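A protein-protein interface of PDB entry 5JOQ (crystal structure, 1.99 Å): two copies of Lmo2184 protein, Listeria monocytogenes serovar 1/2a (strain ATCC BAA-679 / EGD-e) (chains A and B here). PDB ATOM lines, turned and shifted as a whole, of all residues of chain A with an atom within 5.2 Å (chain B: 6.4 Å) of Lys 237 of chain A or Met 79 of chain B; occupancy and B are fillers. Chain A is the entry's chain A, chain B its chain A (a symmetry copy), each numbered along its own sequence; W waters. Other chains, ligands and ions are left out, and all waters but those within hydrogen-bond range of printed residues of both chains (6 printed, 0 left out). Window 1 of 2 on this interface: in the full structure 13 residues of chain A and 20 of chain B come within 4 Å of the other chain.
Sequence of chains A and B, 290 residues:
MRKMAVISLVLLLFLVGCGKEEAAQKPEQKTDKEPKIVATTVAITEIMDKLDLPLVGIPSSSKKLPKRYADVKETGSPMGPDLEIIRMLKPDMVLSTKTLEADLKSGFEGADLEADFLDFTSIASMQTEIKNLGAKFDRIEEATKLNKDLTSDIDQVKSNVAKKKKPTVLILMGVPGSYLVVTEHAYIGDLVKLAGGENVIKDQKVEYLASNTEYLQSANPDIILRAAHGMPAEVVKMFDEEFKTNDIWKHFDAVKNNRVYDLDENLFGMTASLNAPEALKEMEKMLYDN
Of the 13 printed residues of chain B, 6 touch a printed residue of chain A.
Printed residues of chain B that touch a printed residue of chain A: Ser 77, Met 79, Thr 99, Asp 103, Met 173 and Met 270.
Along chain A the printed residues that touch a printed residue of chain B span positions 233 to 241.
The side-chain carboxylate (OD2) of Asp 240 of chain A is in salt-bridge range of the side-chain amino group (NZ) of Lys 237 of chain A.
NZ of Lys 237 of chain A lies within salt-bridge range of OE2 of Glu 241 of chain A (3.8 Å).
OE1 of Glu 241 of chain A lies within salt-bridge range of NZ of Lys 244 of chain A (3.1 Å).
N of Met 79 of chain B is in hydrogen-bond range of OG of Ser 77 of chain B, 3.0 Å away.
Of chain B, only Met 79, Thr 99 and Asp 103 come within 4 Å of Lys 237 of chain A.
Printed residues of chain A within 4 Å of Met 79 of chain B: Ala 233 and Lys 237.
Of the printed residues of chain B, Met 238 of chain A touches Met 173 (3.7 Å).
Of the printed residues of chain A, Thr 99 of chain B touches Lys 237 (3.6 Å) and Glu 241 (3.7 Å).
Printed residues of chain A within 4 Å of Met 270 of chain B: Glu 241.
Lys 244 of chain A touches none of the printed residues of chain B.
Asp 240 of chain A touches none of the printed residues of chain B.
The nearest residue of chain B that does not touch Lys 237 of chain A is Leu 100 of chain B (4.02 Å).
The nearest residue of chain A that does not touch Met 79 of chain B is Glu 234 of chain A (4.05 Å).
The nearest printed residue of chain A that does not touch Ser 77 of chain B is Glu 234 of chain A (6.6 Å).
Ser 77 of chain B touches Ala 233 of chain A (OG to CB, 3.96 Å).
CG of Met 79 of chain B touches O of Ala 233 of chain A, 3.8 Å away.
Lys 237 of chain A touches Met 79 of chain B.
Thr 99 of chain B touches Lys 237 of chain A (O to NZ, 3.6 Å).
CG of Met 173 of chain B touches SD of Met 238 of chain A, at 3.7 Å.
Glu 241 of chain A touches Thr 99 of chain B (OE2 to CG2, 3.7 Å).
CE of Met 270 of chain B touches OE2 of Glu 241 of chain A (3.9 Å).
No position is printed for both chains.
Of the 8 pairs that touch across the chains among the printed residues, none has its exchanged pair printed and touching as well.
Water W1 lies within hydrogen-bond range of the side-chain carboxylate of Glu 234 of chain A (2.5 Å) and the backbone NH of Met 270 of chain B (2.9 Å).
Water W3 lies within hydrogen-bond range of the side-chain carboxylate (OE2) of Glu 241 of chain A (2.5 Å), the backbone carbonyl oxygen (O) of Thr 99 of chain B (2.8 Å), the side-chain amino group (NZ) of Lys 244 of chain A (3.0 Å) and the side-chain amino group (NZ) of Lys 237 of chain A (3.1 Å).
Water W2 lies within hydrogen-bond range of the side-chain carboxylate of Asp 240 of chain A, the side-chain carboxylate of Asp 103 of chain B, the side-chain amino group of Lys 237 of chain A and the side-chain amino group of Lys 244 of chain A.
Water W5 bridges OD1 of Asp 240 of chain A and OD1 of Asp 103 of chain B.
Water W4 lies within hydrogen-bond range of O of Thr 99 of chain B (2.9 Å), N of Asp 103 of chain B (2.9 Å) and NZ of Lys 237 of chain A (3.3 Å).
Water W6 lies within hydrogen-bond range of the backbone carbonyl oxygen (O) of Glu 234 of chain A (3.0 Å) and the side-chain sulfur (SD) of Met 270 of chain B (3.3 Å).
The side-chain carboxylate (OD2) of Asp 103 of chain B lies within salt-bridge range of the side-chain amino group (NZ) of Lys 237 of chain A, at 3.1 Å.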
ATOM      1  N   ALA A 233       1.194 -19.175 -17.027  1.00  0.00           N
ATOM      2  CA  ALA A 233       0.296 -18.492 -16.102  1.00  0.00           C
ATOM      3  C   ALA A 233      -0.908 -19.364 -15.769  1.00  0.00           C
ATOM      4  O   ALA A 233      -1.479 -19.266 -14.673  1.00  0.00           O
ATOM      5  CB  ALA A 233      -0.165 -17.177 -16.731  1.00  0.00           C
ATOM      6  N   GLU A 234      -1.371 -20.145 -16.744  1.00  0.00           N
ATOM      7  CA  GLU A 234      -2.509 -21.016 -16.504  1.00  0.00           C
ATOM      8  C   GLU A 234      -2.178 -22.038 -15.419  1.00  0.00           C
ATOM      9  O   GLU A 234      -3.015 -22.347 -14.567  1.00  0.00           O
ATOM     10  CB  GLU A 234      -2.915 -21.644 -17.843  1.00  0.00           C
ATOM     11  CG  GLU A 234      -4.110 -22.415 -17.826  1.00  0.00           C
ATOM     12  CD  GLU A 234      -4.543 -22.894 -19.218  1.00  0.00           C
ATOM     13  OE1 GLU A 234      -3.792 -22.785 -20.231  1.00  0.00           O
ATOM     14  OE2 GLU A 234      -5.653 -23.432 -19.286  1.00  0.00           O
ATOM     15  N   VAL A 235      -0.929 -22.523 -15.385  1.00  0.00           N
ATOM     16  CA  VAL A 235      -0.513 -23.426 -14.314  1.00  0.00           C
ATOM     17  C   VAL A 235      -0.464 -22.683 -12.985  1.00  0.00           C
ATOM     18  O   VAL A 235      -0.892 -23.198 -11.940  1.00  0.00           O
ATOM     19  CB  VAL A 235       0.865 -24.050 -14.631  1.00  0.00           C
ATOM     20  CG1 VAL A 235       1.376 -24.775 -13.425  1.00  0.00           C
ATOM     21  CG2 VAL A 235       0.778 -24.983 -15.861  1.00  0.00           C
ATOM     22  N   VAL A 236       0.056 -21.471 -12.996  1.00  0.00           N
ATOM     23  CA  VAL A 236       0.167 -20.691 -11.779  1.00  0.00           C
ATOM     24  C   VAL A 236      -1.212 -20.439 -11.151  1.00  0.00           C
ATOM     25  O   VAL A 236      -1.344 -20.428  -9.960  1.00  0.00           O
ATOM     26  CB  VAL A 236       0.933 -19.378 -12.012  1.00  0.00           C
ATOM     27  CG1 VAL A 236       0.895 -18.502 -10.762  1.00  0.00           C
ATOM     28  CG2 VAL A 236       2.364 -19.674 -12.438  1.00  0.00           C
ATOM     29  N   LYS A 237      -2.218 -20.237 -11.982  1.00  0.00           N
ATOM     30  CA  LYS A 237      -3.565 -20.025 -11.480  1.00  0.00           C
ATOM     31  C   LYS A 237      -4.041 -21.256 -10.724  1.00  0.00           C
ATOM     32  O   LYS A 237      -4.632 -21.158  -9.697  1.00  0.00           O
ATOM     33  CB  LYS A 237      -4.541 -19.666 -12.590  1.00  0.00           C
ATOM     34  CG  LYS A 237      -5.932 -19.336 -12.082  1.00  0.00           C
ATOM     35  CD  LYS A 237      -5.908 -18.342 -10.940  1.00  0.00           C
ATOM     36  CE  LYS A 237      -7.293 -18.098 -10.365  1.00  0.00           C
ATOM     37  NZ  LYS A 237      -7.339 -17.171  -9.212  1.00  0.00           N
ATOM     38  N   MET A 238      -3.737 -22.422 -11.253  1.00  0.00           N
ATOM     39  CA  MET A 238      -4.097 -23.674 -10.642  1.00  0.00           C
ATOM     40  C   MET A 238      -3.410 -23.759  -9.270  1.00  0.00           C
ATOM     41  O   MET A 238      -4.002 -24.169  -8.297  1.00  0.00           O
ATOM     42  CB  MET A 238      -3.640 -24.790 -11.581  1.00  0.00           C
ATOM     43  CG  MET A 238      -3.896 -26.212 -11.172  1.00  0.00           C
ATOM     44  SD  MET A 238      -3.699 -27.364 -12.550  1.00  0.00           S
ATOM     45  CE  MET A 238      -1.990 -27.174 -12.992  1.00  0.00           C
ATOM     46  N   PHE A 239      -2.154 -23.335  -9.208  1.00  0.00           N
ATOM     47  CA  PHE A 239      -1.422 -23.357  -7.958  1.00  0.00           C
ATOM     48  C   PHE A 239      -2.114 -22.428  -6.962  1.00  0.00           C
ATOM     49  O   PHE A 239      -2.212 -22.742  -5.812  1.00  0.00           O
ATOM     50  CB  PHE A 239       0.019 -22.885  -8.123  1.00  0.00           C
ATOM     51  CG  PHE A 239       0.913 -23.816  -8.904  1.00  0.00           C
ATOM     52  CD1 PHE A 239       0.552 -25.115  -9.217  1.00  0.00           C
ATOM     53  CD2 PHE A 239       2.154 -23.373  -9.297  1.00  0.00           C
ATOM     54  CE1 PHE A 239       1.414 -25.919  -9.931  1.00  0.00           C
ATOM     55  CE2 PHE A 239       3.013 -24.171 -10.000  1.00  0.00           C
ATOM     56  CZ  PHE A 239       2.645 -25.449 -10.312  1.00  0.00           C
ATOM     57  N   ASP A 240      -2.584 -21.287  -7.449  1.00  0.00           N
ATOM     58  CA  ASP A 240      -3.275 -20.304  -6.602  1.00  0.00           C
ATOM     59  C   ASP A 240      -4.476 -20.944  -5.930  1.00  0.00           C
ATOM     60  O   ASP A 240      -4.711 -20.753  -4.725  1.00  0.00           O
ATOM     61  CB  ASP A 240      -3.704 -19.084  -7.433  1.00  0.00           C
ATOM     62  CG  ASP A 240      -4.602 -18.108  -6.631  1.00  0.00           C
ATOM     63  OD1 ASP A 240      -4.125 -17.559  -5.622  1.00  0.00           O
ATOM     64  OD2 ASP A 240      -5.794 -17.968  -6.994  1.00  0.00           O
ATOM     65  N   GLU A 241      -5.285 -21.689  -6.704  1.00  0.00           N
ATOM     66  CA  GLU A 241      -6.411 -22.388  -6.091  1.00  0.00           C
ATOM     67  C   GLU A 241      -5.942 -23.400  -5.043  1.00  0.00           C
ATOM     68  O   GLU A 241      -6.615 -23.605  -4.032  1.00  0.00           O
ATOM     69  CB  GLU A 241      -7.254 -23.128  -7.143  1.00  0.00           C
ATOM     70  CG  GLU A 241      -7.840 -22.264  -8.213  1.00  0.00           C
ATOM     71  CD  GLU A 241      -8.941 -21.323  -7.736  1.00  0.00           C
ATOM     72  OE1 GLU A 241      -9.544 -21.494  -6.648  1.00  0.00           O
ATOM     73  OE2 GLU A 241      -9.224 -20.404  -8.510  1.00  0.00           O
ATOM     74  N   LYS A 244      -4.982 -21.784  -1.468  1.00  0.00           N
ATOM     75  CA  LYS A 244      -6.125 -21.395  -0.645  1.00  0.00           C
ATOM     76  C   LYS A 244      -6.777 -22.559   0.094  1.00  0.00           C
ATOM     77  O   LYS A 244      -7.521 -22.319   1.057  1.00  0.00           O
ATOM     78  CB  LYS A 244      -7.212 -20.720  -1.514  1.00  0.00           C
ATOM     79  CG  LYS A 244      -6.744 -19.444  -2.211  1.00  0.00           C
ATOM     80  CD  LYS A 244      -7.885 -18.755  -3.005  1.00  0.00           C
ATOM     81  CE  LYS A 244      -8.093 -19.348  -4.388  1.00  0.00           C
ATOM     82  NZ  LYS A 244      -9.287 -18.763  -5.101  1.00  0.00           N
ATOM     83  N   THR B  40     -10.248  -9.936 -22.092  1.00  0.00           N
ATOM     84  CA  THR B  40      -8.975 -10.333 -21.487  1.00  0.00           C
ATOM     85  C   THR B  40      -8.716 -11.840 -21.496  1.00  0.00           C
ATOM     86  O   THR B  40      -7.698 -12.272 -20.948  1.00  0.00           O
ATOM     87  CB  THR B  40      -8.849  -9.844 -20.041  1.00  0.00           C
ATOM     88  OG1 THR B  40      -9.825 -10.522 -19.246  1.00  0.00           O
ATOM     89  CG2 THR B  40      -9.089  -8.337 -19.944  1.00  0.00           C
ATOM     90  N   GLY B  76      -1.957  -8.036 -22.582  1.00  0.00           N
ATOM     91  CA  GLY B  76      -1.226  -8.752 -21.550  1.00  0.00           C
ATOM     92  C   GLY B  76      -1.903 -10.041 -21.120  1.00  0.00           C
ATOM     93  O   GLY B  76      -2.894 -10.490 -21.696  1.00  0.00           O
ATOM     94  N   SER B  77      -1.346 -10.639 -20.075  1.00  0.00           N
ATOM     95  CA  SER B  77      -1.769 -11.969 -19.650  1.00  0.00           C
ATOM     96  C   SER B  77      -3.209 -11.951 -19.159  1.00  0.00           C
ATOM     97  O   SER B  77      -3.580 -11.065 -18.381  1.00  0.00           O
ATOM     98  CB  SER B  77      -0.884 -12.489 -18.525  1.00  0.00           C
ATOM     99  OG  SER B  77      -1.470 -13.649 -17.968  1.00  0.00           O
ATOM    100  N   PRO B  78      -4.039 -12.918 -19.562  1.00  0.00           N
ATOM    101  CA  PRO B  78      -5.380 -13.039 -18.963  1.00  0.00           C
ATOM    102  C   PRO B  78      -5.358 -13.112 -17.454  1.00  0.00           C
ATOM    103  O   PRO B  78      -6.319 -12.677 -16.809  1.00  0.00           O
ATOM    104  CB  PRO B  78      -5.908 -14.350 -19.556  1.00  0.00           C
ATOM    105  CG  PRO B  78      -5.154 -14.484 -20.859  1.00  0.00           C
ATOM    106  CD  PRO B  78      -3.769 -13.979 -20.546  1.00  0.00           C
ATOM    107  N   MET B  79      -4.297 -13.676 -16.866  1.00  0.00           N
ATOM    108  CA  MET B  79      -4.247 -13.871 -15.422  1.00  0.00           C
ATOM    109  C   MET B  79      -3.738 -12.629 -14.704  1.00  0.00           C
ATOM    110  O   MET B  79      -3.604 -12.653 -13.475  1.00  0.00           O
ATOM    111  CB  MET B  79      -3.348 -15.091 -15.073  1.00  0.00           C
ATOM    112  CG  MET B  79      -3.800 -16.428 -15.701  1.00  0.00           C
ATOM    113  SD  MET B  79      -5.435 -16.906 -15.093  1.00  0.00           S
ATOM    114  CE  MET B  79      -5.639 -18.530 -15.862  1.00  0.00           C
ATOM    115  N   GLY B  80      -3.424 -11.571 -15.453  1.00  0.00           N
ATOM    116  CA  GLY B  80      -2.961 -10.316 -14.915  1.00  0.00           C
ATOM    117  C   GLY B  80      -2.784  -9.291 -16.023  1.00  0.00           C
ATOM    118  O   GLY B  80      -1.663  -8.994 -16.437  1.00  0.00           O
ATOM    119  N   PRO B  81      -3.883  -8.759 -16.556  1.00  0.00           N
ATOM    120  CA  PRO B  81      -3.775  -7.896 -17.738  1.00  0.00           C
ATOM    121  C   PRO B  81      -2.977  -6.644 -17.415  1.00  0.00           C
ATOM    122  O   PRO B  81      -2.859  -6.242 -16.255  1.00  0.00           O
ATOM    123  CB  PRO B  81      -5.233  -7.563 -18.072  1.00  0.00           C
ATOM    124  CG  PRO B  81      -6.028  -8.769 -17.508  1.00  0.00           C
ATOM    125  CD  PRO B  81      -5.286  -9.051 -16.207  1.00  0.00           C
ATOM    126  N   THR B  99     -13.816 -16.264 -11.850  1.00  0.00           N
ATOM    127  CA  THR B  99     -12.742 -16.981 -11.157  1.00  0.00           C
ATOM    128  C   THR B  99     -11.515 -16.097 -10.955  1.00  0.00           C
ATOM    129  O   THR B  99     -10.748 -16.308 -10.005  1.00  0.00           O
ATOM    130  CB  THR B  99     -12.413 -18.271 -11.934  1.00  0.00           C
ATOM    131  OG1 THR B  99     -13.555 -19.167 -11.853  1.00  0.00           O
ATOM    132  CG2 THR B  99     -11.134 -18.966 -11.359  1.00  0.00           C
ATOM    133  N   LEU B 100     -11.328 -15.084 -11.808  1.00  0.00           N
ATOM    134  CA  LEU B 100     -10.252 -14.114 -11.650  1.00  0.00           C
ATOM    135  C   LEU B 100     -10.654 -12.845 -10.896  1.00  0.00           C
ATOM    136  O   LEU B 100      -9.812 -11.970 -10.713  1.00  0.00           O
ATOM    137  CB  LEU B 100      -9.699 -13.720 -13.032  1.00  0.00           C
ATOM    138  CG  LEU B 100      -8.516 -14.587 -13.483  1.00  0.00           C
ATOM    139  CD1 LEU B 100      -7.246 -14.310 -12.595  1.00  0.00           C
ATOM    140  CD2 LEU B 100      -8.889 -16.068 -13.448  1.00  0.00           C
ATOM    141  N   ASP B 103      -8.560 -11.763  -7.802  1.00  0.00           N
ATOM    142  CA  ASP B 103      -7.258 -11.304  -8.205  1.00  0.00           C
ATOM    143  C   ASP B 103      -7.197  -9.941  -8.891  1.00  0.00           C
ATOM    144  O   ASP B 103      -6.319  -9.160  -8.621  1.00  0.00           O
ATOM    145  CB  ASP B 103      -6.611 -12.309  -9.147  1.00  0.00           C
ATOM    146  CG  ASP B 103      -6.182 -13.571  -8.445  1.00  0.00           C
ATOM    147  OD1 ASP B 103      -6.225 -13.594  -7.210  1.00  0.00           O
ATOM    148  OD2 ASP B 103      -5.816 -14.525  -9.139  1.00  0.00           O
ATOM    149  N   LEU B 104      -8.130  -9.693  -9.800  1.00  0.00           N
ATOM    150  CA  LEU B 104      -8.102  -8.482 -10.616  1.00  0.00           C
ATOM    151  C   LEU B 104      -9.011  -7.305 -10.341  1.00  0.00           C
ATOM    152  O   LEU B 104      -8.779  -6.237 -10.882  1.00  0.00           O
ATOM    153  CB  LEU B 104      -8.333  -8.878 -12.075  1.00  0.00           C
ATOM    154  CG  LEU B 104      -7.593 -10.082 -12.618  1.00  0.00           C
ATOM    155  CD1 LEU B 104      -7.947 -10.393 -14.061  1.00  0.00           C
ATOM    156  CD2 LEU B 104      -6.110  -9.853 -12.459  1.00  0.00           C
ATOM    157  N   MET B 173      -7.356 -31.934  -9.983  1.00  0.00           N
ATOM    158  CA  MET B 173      -6.719 -30.837 -10.694  1.00  0.00           C
ATOM    159  C   MET B 173      -5.394 -30.542  -9.998  1.00  0.00           C
ATOM    160  O   MET B 173      -5.385 -30.311  -8.792  1.00  0.00           O
ATOM    161  CB  MET B 173      -7.613 -29.565 -10.668  1.00  0.00           C
ATOM    162  CG  MET B 173      -6.996 -28.409 -11.350  1.00  0.00           C
ATOM    163  SD  MET B 173      -7.970 -26.889 -11.236  1.00  0.00           S
ATOM    164  CE  MET B 173      -7.843 -26.385  -9.510  1.00  0.00           C
ATOM    165  N   MET B 270      -9.856 -24.740 -17.120  1.00  0.00           N
ATOM    166  CA  MET B 270     -10.383 -24.641 -15.760  1.00  0.00           C
ATOM    167  C   MET B 270     -11.797 -24.059 -15.748  1.00  0.00           C
ATOM    168  O   MET B 270     -12.587 -24.383 -14.852  1.00  0.00           O
ATOM    169  CB  MET B 270      -9.467 -23.773 -14.893  1.00  0.00           C
ATOM    170  CG  MET B 270      -9.459 -24.196 -13.433  1.00  0.00           C
ATOM    171  SD  MET B 270      -8.182 -23.323 -12.456  1.00  0.00           S
ATOM    172  CE  MET B 270      -9.136 -21.842 -12.098  1.00  0.00           C
HETATM  173  O   HOH W   1      -7.503 -23.164 -17.623  1.00  0.00           O
HETATM  174  O   HOH W   2      -7.498 -16.004  -6.146  1.00  0.00           O
HETATM  175  O   HOH W   3     -10.036 -18.101  -7.956  1.00  0.00           O
HETATM  176  O   HOH W   4      -9.210 -14.527  -8.379  1.00  0.00           O
HETATM  177  O   HOH W   5      -4.192 -14.780  -5.312  1.00  0.00           O
HETATM  178  O   HOH W   6      -5.969 -22.445 -14.791  1.00  0.00           O
